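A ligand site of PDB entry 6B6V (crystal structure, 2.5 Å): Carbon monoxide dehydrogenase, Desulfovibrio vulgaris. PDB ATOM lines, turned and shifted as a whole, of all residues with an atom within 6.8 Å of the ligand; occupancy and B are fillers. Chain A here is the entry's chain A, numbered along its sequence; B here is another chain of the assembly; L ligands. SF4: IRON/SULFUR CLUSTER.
The backbone NH (N) of Met 64 lies close to the side-chain sulfur (SG) of Cys 62, 3.4 Å away. O of Cys 59 is in hydrogen-bond range of N of Cys 67 (2.9 Å). SG of Cys 59 lies close to N of Asn 61, at 3.6 Å. The backbone NH (N) of Ala 84 lies close to the side-chain sulfur (SG) of Cys 82 (3.6 Å). The side-chain sulfur (SG) of Cys 67 sits close to the backbone NH (N) of Val 81, at 3.4 Å. O of Cys 67 lies within hydrogen-bond range of OG1 of Thr 58. The side-chain sulfur (SD) of Met 211 sits close to the side-chain hydroxyl (OH) of Tyr 561 of chain B (3.5 Å). The backbone carbonyl oxygen (O) of Thr 209 lies close to the side-chain amide oxygen (OD1) of Asn 61 (2.8 Å).
N of Cys 62 sits close to S3 of the ligand. FE4 of the ligand is bound by SG of Cys 62. SG of Cys 59 binds FE1 of the ligand, at 2.3 Å. S1 of the ligand sits close to N of Cys 82. The side-chain sulfur (SG) of Cys 82 binds an iron atom (FE3) of the ligand (2.3 Å). FE2 of the ligand is bound by SG of Cys 67 (2.3 Å). S2 of the ligand sits close to NH2 of Arg 92 (3.6 Å). A sulfur (S1) of the ligand lies close to the backbone NH (N) of Val 81 (3.7 Å). N of Asn 61 sits close to S3 of the ligand (3.8 Å).
Merely in contact with the ligand: Met 211, Ile 89, Gly 65, Met 64 and Gly 80. The nearest printed residue that does not touch the ligand is Pro 66 (4.2 Å).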
ATOM      1  N   THR A  58     -14.818   3.332  11.799  1.00  0.00           N
ATOM      2  CA  THR A  58     -13.495   3.671  11.312  1.00  0.00           C
ATOM      3  C   THR A  58     -13.110   2.664  10.246  1.00  0.00           C
ATOM      4  O   THR A  58     -13.528   1.508  10.277  1.00  0.00           O
ATOM      5  CB  THR A  58     -12.446   3.697  12.439  1.00  0.00           C
ATOM      6  OG1 THR A  58     -11.136   3.855  11.871  1.00  0.00           O
ATOM      7  CG2 THR A  58     -12.508   2.420  13.244  1.00  0.00           C
ATOM      8  N   CYS A  59     -12.315   3.119   9.276  1.00  0.00           N
ATOM      9  CA  CYS A  59     -11.949   2.279   8.147  1.00  0.00           C
ATOM     10  C   CYS A  59     -10.496   2.496   7.782  1.00  0.00           C
ATOM     11  O   CYS A  59     -10.033   3.647   7.723  1.00  0.00           O
ATOM     12  CB  CYS A  59     -12.859   2.587   6.940  1.00  0.00           C
ATOM     13  SG  CYS A  59     -12.659   1.448   5.544  1.00  0.00           S
ATOM     14  N   ARG A  60      -9.772   1.394   7.559  1.00  0.00           N
ATOM     15  CA  ARG A  60      -8.374   1.403   7.145  1.00  0.00           C
ATOM     16  C   ARG A  60      -8.154   0.642   5.849  1.00  0.00           C
ATOM     17  O   ARG A  60      -7.021   0.225   5.557  1.00  0.00           O
ATOM     18  CB  ARG A  60      -7.467   0.835   8.238  1.00  0.00           C
ATOM     19  CG  ARG A  60      -7.642   1.467   9.596  1.00  0.00           C
ATOM     20  CD  ARG A  60      -6.596   0.933  10.582  1.00  0.00           C
ATOM     21  NE  ARG A  60      -6.756  -0.498  10.839  1.00  0.00           N
ATOM     22  CZ  ARG A  60      -7.370  -0.998  11.908  1.00  0.00           C
ATOM     23  NH1 ARG A  60      -7.906  -0.196  12.818  1.00  0.00           N
ATOM     24  NH2 ARG A  60      -7.460  -2.319  12.057  1.00  0.00           N
ATOM     25  N   ASN A  61      -9.207   0.438   5.051  1.00  0.00           N
ATOM     26  CA  ASN A  61      -9.151  -0.479   3.925  1.00  0.00           C
ATOM     27  C   ASN A  61      -8.385   0.071   2.726  1.00  0.00           C
ATOM     28  O   ASN A  61      -8.162  -0.676   1.770  1.00  0.00           O
ATOM     29  CB  ASN A  61     -10.562  -0.858   3.485  1.00  0.00           C
ATOM     30  CG  ASN A  61     -11.242  -1.825   4.448  1.00  0.00           C
ATOM     31  OD1 ASN A  61     -12.327  -2.337   4.179  1.00  0.00           O
ATOM     32  ND2 ASN A  61     -10.608  -2.066   5.595  1.00  0.00           N
ATOM     33  N   CYS A  62      -7.965   1.336   2.744  1.00  0.00           N
ATOM     34  CA  CYS A  62      -7.127   1.867   1.676  1.00  0.00           C
ATOM     35  C   CYS A  62      -6.404   3.092   2.216  1.00  0.00           C
ATOM     36  O   CYS A  62      -6.694   3.570   3.321  1.00  0.00           O
ATOM     37  CB  CYS A  62      -7.945   2.197   0.431  1.00  0.00           C
ATOM     38  SG  CYS A  62      -8.777   3.784   0.494  1.00  0.00           S
ATOM     39  N   ILE A  63      -5.460   3.598   1.430  1.00  0.00           N
ATOM     40  CA  ILE A  63      -4.649   4.727   1.865  1.00  0.00           C
ATOM     41  C   ILE A  63      -5.100   6.034   1.218  1.00  0.00           C
ATOM     42  O   ILE A  63      -4.349   7.014   1.230  1.00  0.00           O
ATOM     43  CB  ILE A  63      -3.142   4.482   1.661  1.00  0.00           C
ATOM     44  CG1 ILE A  63      -2.780   4.473   0.181  1.00  0.00           C
ATOM     45  CG2 ILE A  63      -2.723   3.176   2.347  1.00  0.00           C
ATOM     46  CD1 ILE A  63      -1.411   5.056  -0.093  1.00  0.00           C
ATOM     47  N   MET A  64      -6.308   6.080   0.656  1.00  0.00           N
ATOM     48  CA  MET A  64      -7.014   7.355   0.607  1.00  0.00           C
ATOM     49  C   MET A  64      -7.460   7.753   2.000  1.00  0.00           C
ATOM     50  O   MET A  64      -7.556   8.951   2.310  1.00  0.00           O
ATOM     51  CB  MET A  64      -8.214   7.295  -0.332  1.00  0.00           C
ATOM     52  CG  MET A  64      -7.872   7.163  -1.808  1.00  0.00           C
ATOM     53  SD  MET A  64      -9.217   7.658  -2.911  1.00  0.00           S
ATOM     54  CE  MET A  64     -10.626   6.841  -2.164  1.00  0.00           C
ATOM     55  N   GLY A  65      -7.718   6.764   2.863  1.00  0.00           N
ATOM     56  CA  GLY A  65      -7.942   6.994   4.260  1.00  0.00           C
ATOM     57  C   GLY A  65      -6.631   6.990   5.030  1.00  0.00           C
ATOM     58  O   GLY A  65      -5.579   7.357   4.490  1.00  0.00           O
ATOM     59  N   PRO A  66      -6.661   6.550   6.301  1.00  0.00           N
ATOM     60  CA  PRO A  66      -7.799   5.979   7.018  1.00  0.00           C
ATOM     61  C   PRO A  66      -8.888   7.009   7.330  1.00  0.00           C
ATOM     62  O   PRO A  66      -8.619   8.207   7.384  1.00  0.00           O
ATOM     63  CB  PRO A  66      -7.171   5.457   8.308  1.00  0.00           C
ATOM     64  CG  PRO A  66      -6.037   6.383   8.544  1.00  0.00           C
ATOM     65  CD  PRO A  66      -5.481   6.665   7.172  1.00  0.00           C
ATOM     66  N   CYS A  67     -10.110   6.526   7.519  1.00  0.00           N
ATOM     67  CA  CYS A  67     -11.269   7.388   7.676  1.00  0.00           C
ATOM     68  C   CYS A  67     -11.993   7.078   8.978  1.00  0.00           C
ATOM     69  O   CYS A  67     -11.904   5.976   9.507  1.00  0.00           O
ATOM     70  CB  CYS A  67     -12.239   7.228   6.484  1.00  0.00           C
ATOM     71  SG  CYS A  67     -11.495   7.560   4.866  1.00  0.00           S
ATOM     72  N   ARG A  68     -12.685   8.091   9.494  1.00  0.00           N
ATOM     73  CA  ARG A  68     -13.593   7.938  10.624  1.00  0.00           C
ATOM     74  C   ARG A  68     -14.899   8.653  10.295  1.00  0.00           C
ATOM     75  O   ARG A  68     -14.897   9.734   9.703  1.00  0.00           O
ATOM     76  CB  ARG A  68     -12.988   8.502  11.906  1.00  0.00           C
ATOM     77  CG  ARG A  68     -11.813   7.713  12.450  1.00  0.00           C
ATOM     78  CD  ARG A  68     -10.967   8.578  13.358  1.00  0.00           C
ATOM     79  NE  ARG A  68     -10.488   9.756  12.636  1.00  0.00           N
ATOM     80  CZ  ARG A  68     -10.055  10.867  13.214  1.00  0.00           C
ATOM     81  NH1 ARG A  68     -10.047  10.966  14.541  1.00  0.00           N
ATOM     82  NH2 ARG A  68      -9.637  11.884  12.477  1.00  0.00           N
ATOM     83  N   ILE A  69     -16.019   8.020  10.657  1.00  0.00           N
ATOM     84  CA  ILE A  69     -17.339   8.630  10.502  1.00  0.00           C
ATOM     85  C   ILE A  69     -17.755   9.181  11.853  1.00  0.00           C
ATOM     86  O   ILE A  69     -17.842   8.445  12.847  1.00  0.00           O
ATOM     87  CB  ILE A  69     -18.368   7.616   9.964  1.00  0.00           C
ATOM     88  CG1 ILE A  69     -17.839   6.947   8.703  1.00  0.00           C
ATOM     89  CG2 ILE A  69     -19.672   8.321   9.639  1.00  0.00           C
ATOM     90  CD1 ILE A  69     -17.544   7.907   7.579  1.00  0.00           C
ATOM     91  N   LEU A  79     -18.877  10.938   5.566  1.00  0.00           N
ATOM     92  CA  LEU A  79     -18.513   9.891   4.623  1.00  0.00           C
ATOM     93  C   LEU A  79     -16.996   9.716   4.629  1.00  0.00           C
ATOM     94  O   LEU A  79     -16.254  10.640   4.949  1.00  0.00           O
ATOM     95  CB  LEU A  79     -18.987  10.211   3.208  1.00  0.00           C
ATOM     96  CG  LEU A  79     -20.445  10.617   3.050  1.00  0.00           C
ATOM     97  CD1 LEU A  79     -20.688  11.218   1.676  1.00  0.00           C
ATOM     98  CD2 LEU A  79     -21.351   9.411   3.271  1.00  0.00           C
ATOM     99  N   GLY A  80     -16.554   8.520   4.255  1.00  0.00           N
ATOM    100  CA  GLY A  80     -15.144   8.298   3.991  1.00  0.00           C
ATOM    101  C   GLY A  80     -14.714   9.041   2.741  1.00  0.00           C
ATOM    102  O   GLY A  80     -15.495   9.730   2.083  1.00  0.00           O
ATOM    103  N   VAL A  81     -13.429   8.885   2.402  1.00  0.00           N
ATOM    104  CA  VAL A  81     -12.907   9.590   1.231  1.00  0.00           C
ATOM    105  C   VAL A  81     -13.520   9.030  -0.040  1.00  0.00           C
ATOM    106  O   VAL A  81     -13.862   9.784  -0.965  1.00  0.00           O
ATOM    107  CB  VAL A  81     -11.364   9.505   1.203  1.00  0.00           C
ATOM    108  CG1 VAL A  81     -10.828  10.171  -0.064  1.00  0.00           C
ATOM    109  CG2 VAL A  81     -10.776  10.154   2.437  1.00  0.00           C
ATOM    110  N   CYS A  82     -13.690   7.710  -0.112  1.00  0.00           N
ATOM    111  CA  CYS A  82     -14.334   7.084  -1.269  1.00  0.00           C
ATOM    112  C   CYS A  82     -15.832   7.370  -1.331  1.00  0.00           C
ATOM    113  O   CYS A  82     -16.436   7.150  -2.381  1.00  0.00           O
ATOM    114  CB  CYS A  82     -14.113   5.571  -1.233  1.00  0.00           C
ATOM    115  SG  CYS A  82     -14.847   4.725   0.187  1.00  0.00           S
ATOM    116  N   GLY A  83     -16.435   7.862  -0.243  1.00  0.00           N
ATOM    117  CA  GLY A  83     -17.860   8.135  -0.212  1.00  0.00           C
ATOM    118  C   GLY A  83     -18.666   7.154   0.591  1.00  0.00           C
ATOM    119  O   GLY A  83     -19.890   7.322   0.702  1.00  0.00           O
ATOM    120  N   ALA A  84     -18.041   6.134   1.163  1.00  0.00           N
ATOM    121  CA  ALA A  84     -18.763   5.162   1.979  1.00  0.00           C
ATOM    122  C   ALA A  84     -19.324   5.820   3.229  1.00  0.00           C
ATOM    123  O   ALA A  84     -18.645   6.599   3.906  1.00  0.00           O
ATOM    124  CB  ALA A  84     -17.839   4.004   2.360  1.00  0.00           C
ATOM    125  N   ASP A  85     -20.589   5.521   3.529  1.00  0.00           N
ATOM    126  CA  ASP A  85     -21.229   6.022   4.731  1.00  0.00           C
ATOM    127  C   ASP A  85     -20.960   5.062   5.899  1.00  0.00           C
ATOM    128  O   ASP A  85     -20.257   4.058   5.757  1.00  0.00           O
ATOM    129  CB  ASP A  85     -22.717   6.224   4.495  1.00  0.00           C
ATOM    130  CG  ASP A  85     -23.437   4.947   4.089  1.00  0.00           C
ATOM    131  OD1 ASP A  85     -22.909   3.854   4.378  1.00  0.00           O
ATOM    132  OD2 ASP A  85     -24.509   5.034   3.461  1.00  0.00           O
ATOM    133  N   ILE A  89     -19.297   1.151   6.037  1.00  0.00           N
ATOM    134  CA  ILE A  89     -18.034   0.971   6.752  1.00  0.00           C
ATOM    135  C   ILE A  89     -18.208  -0.008   7.908  1.00  0.00           C
ATOM    136  O   ILE A  89     -17.377  -0.895   8.113  1.00  0.00           O
ATOM    137  CB  ILE A  89     -17.503   2.342   7.226  1.00  0.00           C
ATOM    138  CG1 ILE A  89     -17.058   3.165   6.026  1.00  0.00           C
ATOM    139  CG2 ILE A  89     -16.361   2.165   8.229  1.00  0.00           C
ATOM    140  CD1 ILE A  89     -16.630   4.558   6.364  1.00  0.00           C
ATOM    141  N   ARG A  92     -18.813  -3.590   6.384  1.00  0.00           N
ATOM    142  CA  ARG A  92     -17.569  -4.181   5.874  1.00  0.00           C
ATOM    143  C   ARG A  92     -16.654  -4.633   7.001  1.00  0.00           C
ATOM    144  O   ARG A  92     -16.037  -5.696   6.913  1.00  0.00           O
ATOM    145  CB  ARG A  92     -16.850  -3.186   4.958  1.00  0.00           C
ATOM    146  CG  ARG A  92     -17.545  -2.932   3.637  1.00  0.00           C
ATOM    147  CD  ARG A  92     -16.682  -2.133   2.696  1.00  0.00           C
ATOM    148  NE  ARG A  92     -16.102  -0.945   3.313  1.00  0.00           N
ATOM    149  CZ  ARG A  92     -15.748   0.145   2.643  1.00  0.00           C
ATOM    150  NH1 ARG A  92     -15.932   0.194   1.324  1.00  0.00           N
ATOM    151  NH2 ARG A  92     -15.216   1.185   3.270  1.00  0.00           N
ATOM    152  N   THR A 209     -15.318  -6.303   0.640  1.00  0.00           N
ATOM    153  CA  THR A 209     -14.918  -5.281   1.590  1.00  0.00           C
ATOM    154  C   THR A 209     -13.767  -4.415   1.091  1.00  0.00           C
ATOM    155  O   THR A 209     -13.376  -3.469   1.788  1.00  0.00           O
ATOM    156  CB  THR A 209     -14.565  -5.943   2.928  1.00  0.00           C
ATOM    157  OG1 THR A 209     -13.616  -6.997   2.720  1.00  0.00           O
ATOM    158  CG2 THR A 209     -15.825  -6.531   3.553  1.00  0.00           C
ATOM    159  N   HIS A 210     -13.218  -4.718  -0.074  1.00  0.00           N
ATOM    160  CA  HIS A 210     -12.304  -3.789  -0.738  1.00  0.00           C
ATOM    161  C   HIS A 210     -13.071  -2.545  -1.165  1.00  0.00           C
ATOM    162  O   HIS A 210     -14.267  -2.589  -1.430  1.00  0.00           O
ATOM    163  CB  HIS A 210     -11.662  -4.460  -1.951  1.00  0.00           C
ATOM    164  CG  HIS A 210     -10.605  -3.638  -2.614  1.00  0.00           C
ATOM    165  ND1 HIS A 210     -10.900  -2.567  -3.437  1.00  0.00           N
ATOM    166  CD2 HIS A 210      -9.253  -3.705  -2.571  1.00  0.00           C
ATOM    167  CE1 HIS A 210      -9.779  -2.021  -3.871  1.00  0.00           C
ATOM    168  NE2 HIS A 210      -8.764  -2.699  -3.361  1.00  0.00           N
ATOM    169  N   MET A 211     -12.356  -1.420  -1.213  1.00  0.00           N
ATOM    170  CA  MET A 211     -12.975  -0.161  -1.618  1.00  0.00           C
ATOM    171  C   MET A 211     -13.653  -0.304  -2.970  1.00  0.00           C
ATOM    172  O   MET A 211     -13.090  -0.892  -3.905  1.00  0.00           O
ATOM    173  CB  MET A 211     -11.936   0.970  -1.683  1.00  0.00           C
ATOM    174  CG  MET A 211     -12.499   2.371  -1.963  1.00  0.00           C
ATOM    175  SD  MET A 211     -13.126   2.715  -3.640  1.00  0.00           S
ATOM    176  CE  MET A 211     -12.032   4.028  -4.179  1.00  0.00           C
ATOM    177  N   GLY A 212     -14.855   0.236  -3.081  1.00  0.00           N
ATOM    178  CA  GLY A 212     -15.526   0.310  -4.367  1.00  0.00           C
ATOM    179  C   GLY A 212     -16.053  -1.005  -4.891  1.00  0.00           C
ATOM    180  O   GLY A 212     -16.187  -1.159  -6.113  1.00  0.00           O
ATOM    181  N   GLN B  46     -11.293  14.333   5.999  1.00  0.00           N
ATOM    182  CA  GLN B  46     -10.628  13.255   6.725  1.00  0.00           C
ATOM    183  C   GLN B  46      -9.167  13.568   7.041  1.00  0.00           C
ATOM    184  O   GLN B  46      -8.389  12.646   7.316  1.00  0.00           O
ATOM    185  CB  GLN B  46     -10.721  11.950   5.940  1.00  0.00           C
ATOM    186  CG  GLN B  46     -12.138  11.432   5.745  1.00  0.00           C
ATOM    187  CD  GLN B  46     -12.784  10.949   7.047  1.00  0.00           C
ATOM    188  OE1 GLN B  46     -12.101  10.653   8.021  1.00  0.00           O
ATOM    189  NE2 GLN B  46     -14.111  10.854   7.053  1.00  0.00           N
ATOM    190  N   PRO B 351     -18.648   4.999  -4.110  1.00  0.00           N
ATOM    191  CA  PRO B 351     -20.106   5.127  -3.916  1.00  0.00           C
ATOM    192  C   PRO B 351     -20.617   6.548  -4.092  1.00  0.00           C
ATOM    193  O   PRO B 351     -21.833   6.737  -4.216  1.00  0.00           O
ATOM    194  CB  PRO B 351     -20.333   4.632  -2.484  1.00  0.00           C
ATOM    195  CG  PRO B 351     -19.090   3.925  -2.113  1.00  0.00           C
ATOM    196  CD  PRO B 351     -17.979   4.502  -2.906  1.00  0.00           C
ATOM    197  N   TYR B 561      -3.351   3.806  -4.098  1.00  0.00           N
ATOM    198  CA  TYR B 561      -4.303   3.939  -3.005  1.00  0.00           C
ATOM    199  C   TYR B 561      -4.804   2.600  -2.493  1.00  0.00           C
ATOM    200  O   TYR B 561      -5.039   2.458  -1.290  1.00  0.00           O
ATOM    201  CB  TYR B 561      -5.518   4.821  -3.417  1.00  0.00           C
ATOM    202  CG  TYR B 561      -6.729   4.010  -3.815  1.00  0.00           C
ATOM    203  CD1 TYR B 561      -7.665   3.600  -2.863  1.00  0.00           C
ATOM    204  CD2 TYR B 561      -6.924   3.619  -5.128  1.00  0.00           C
ATOM    205  CE1 TYR B 561      -8.755   2.831  -3.213  1.00  0.00           C
ATOM    206  CE2 TYR B 561      -8.018   2.855  -5.492  1.00  0.00           C
ATOM    207  CZ  TYR B 561      -8.933   2.463  -4.530  1.00  0.00           C
ATOM    208  OH  TYR B 561     -10.019   1.710  -4.899  1.00  0.00           O
HETATM  209 FE1  SF4 L   1     -12.230   2.953   3.886  1.00  0.00          FE
HETATM  210 FE2  SF4 L   1     -11.730   5.629   3.659  1.00  0.00          FE
HETATM  211 FE3  SF4 L   1     -13.215   4.358   1.748  1.00  0.00          FE
HETATM  212 FE4  SF4 L   1     -10.526   3.853   1.952  1.00  0.00          FE
HETATM  213  S1  SF4 L   1     -11.519   5.841   1.400  1.00  0.00           S
HETATM  214  S2  SF4 L   1     -12.185   2.309   1.707  1.00  0.00           S
HETATM  215  S3  SF4 L   1     -10.234   3.997   4.212  1.00  0.00           S
HETATM  216  S4  SF4 L   1     -13.763   4.650   3.935  1.00  0.00           S
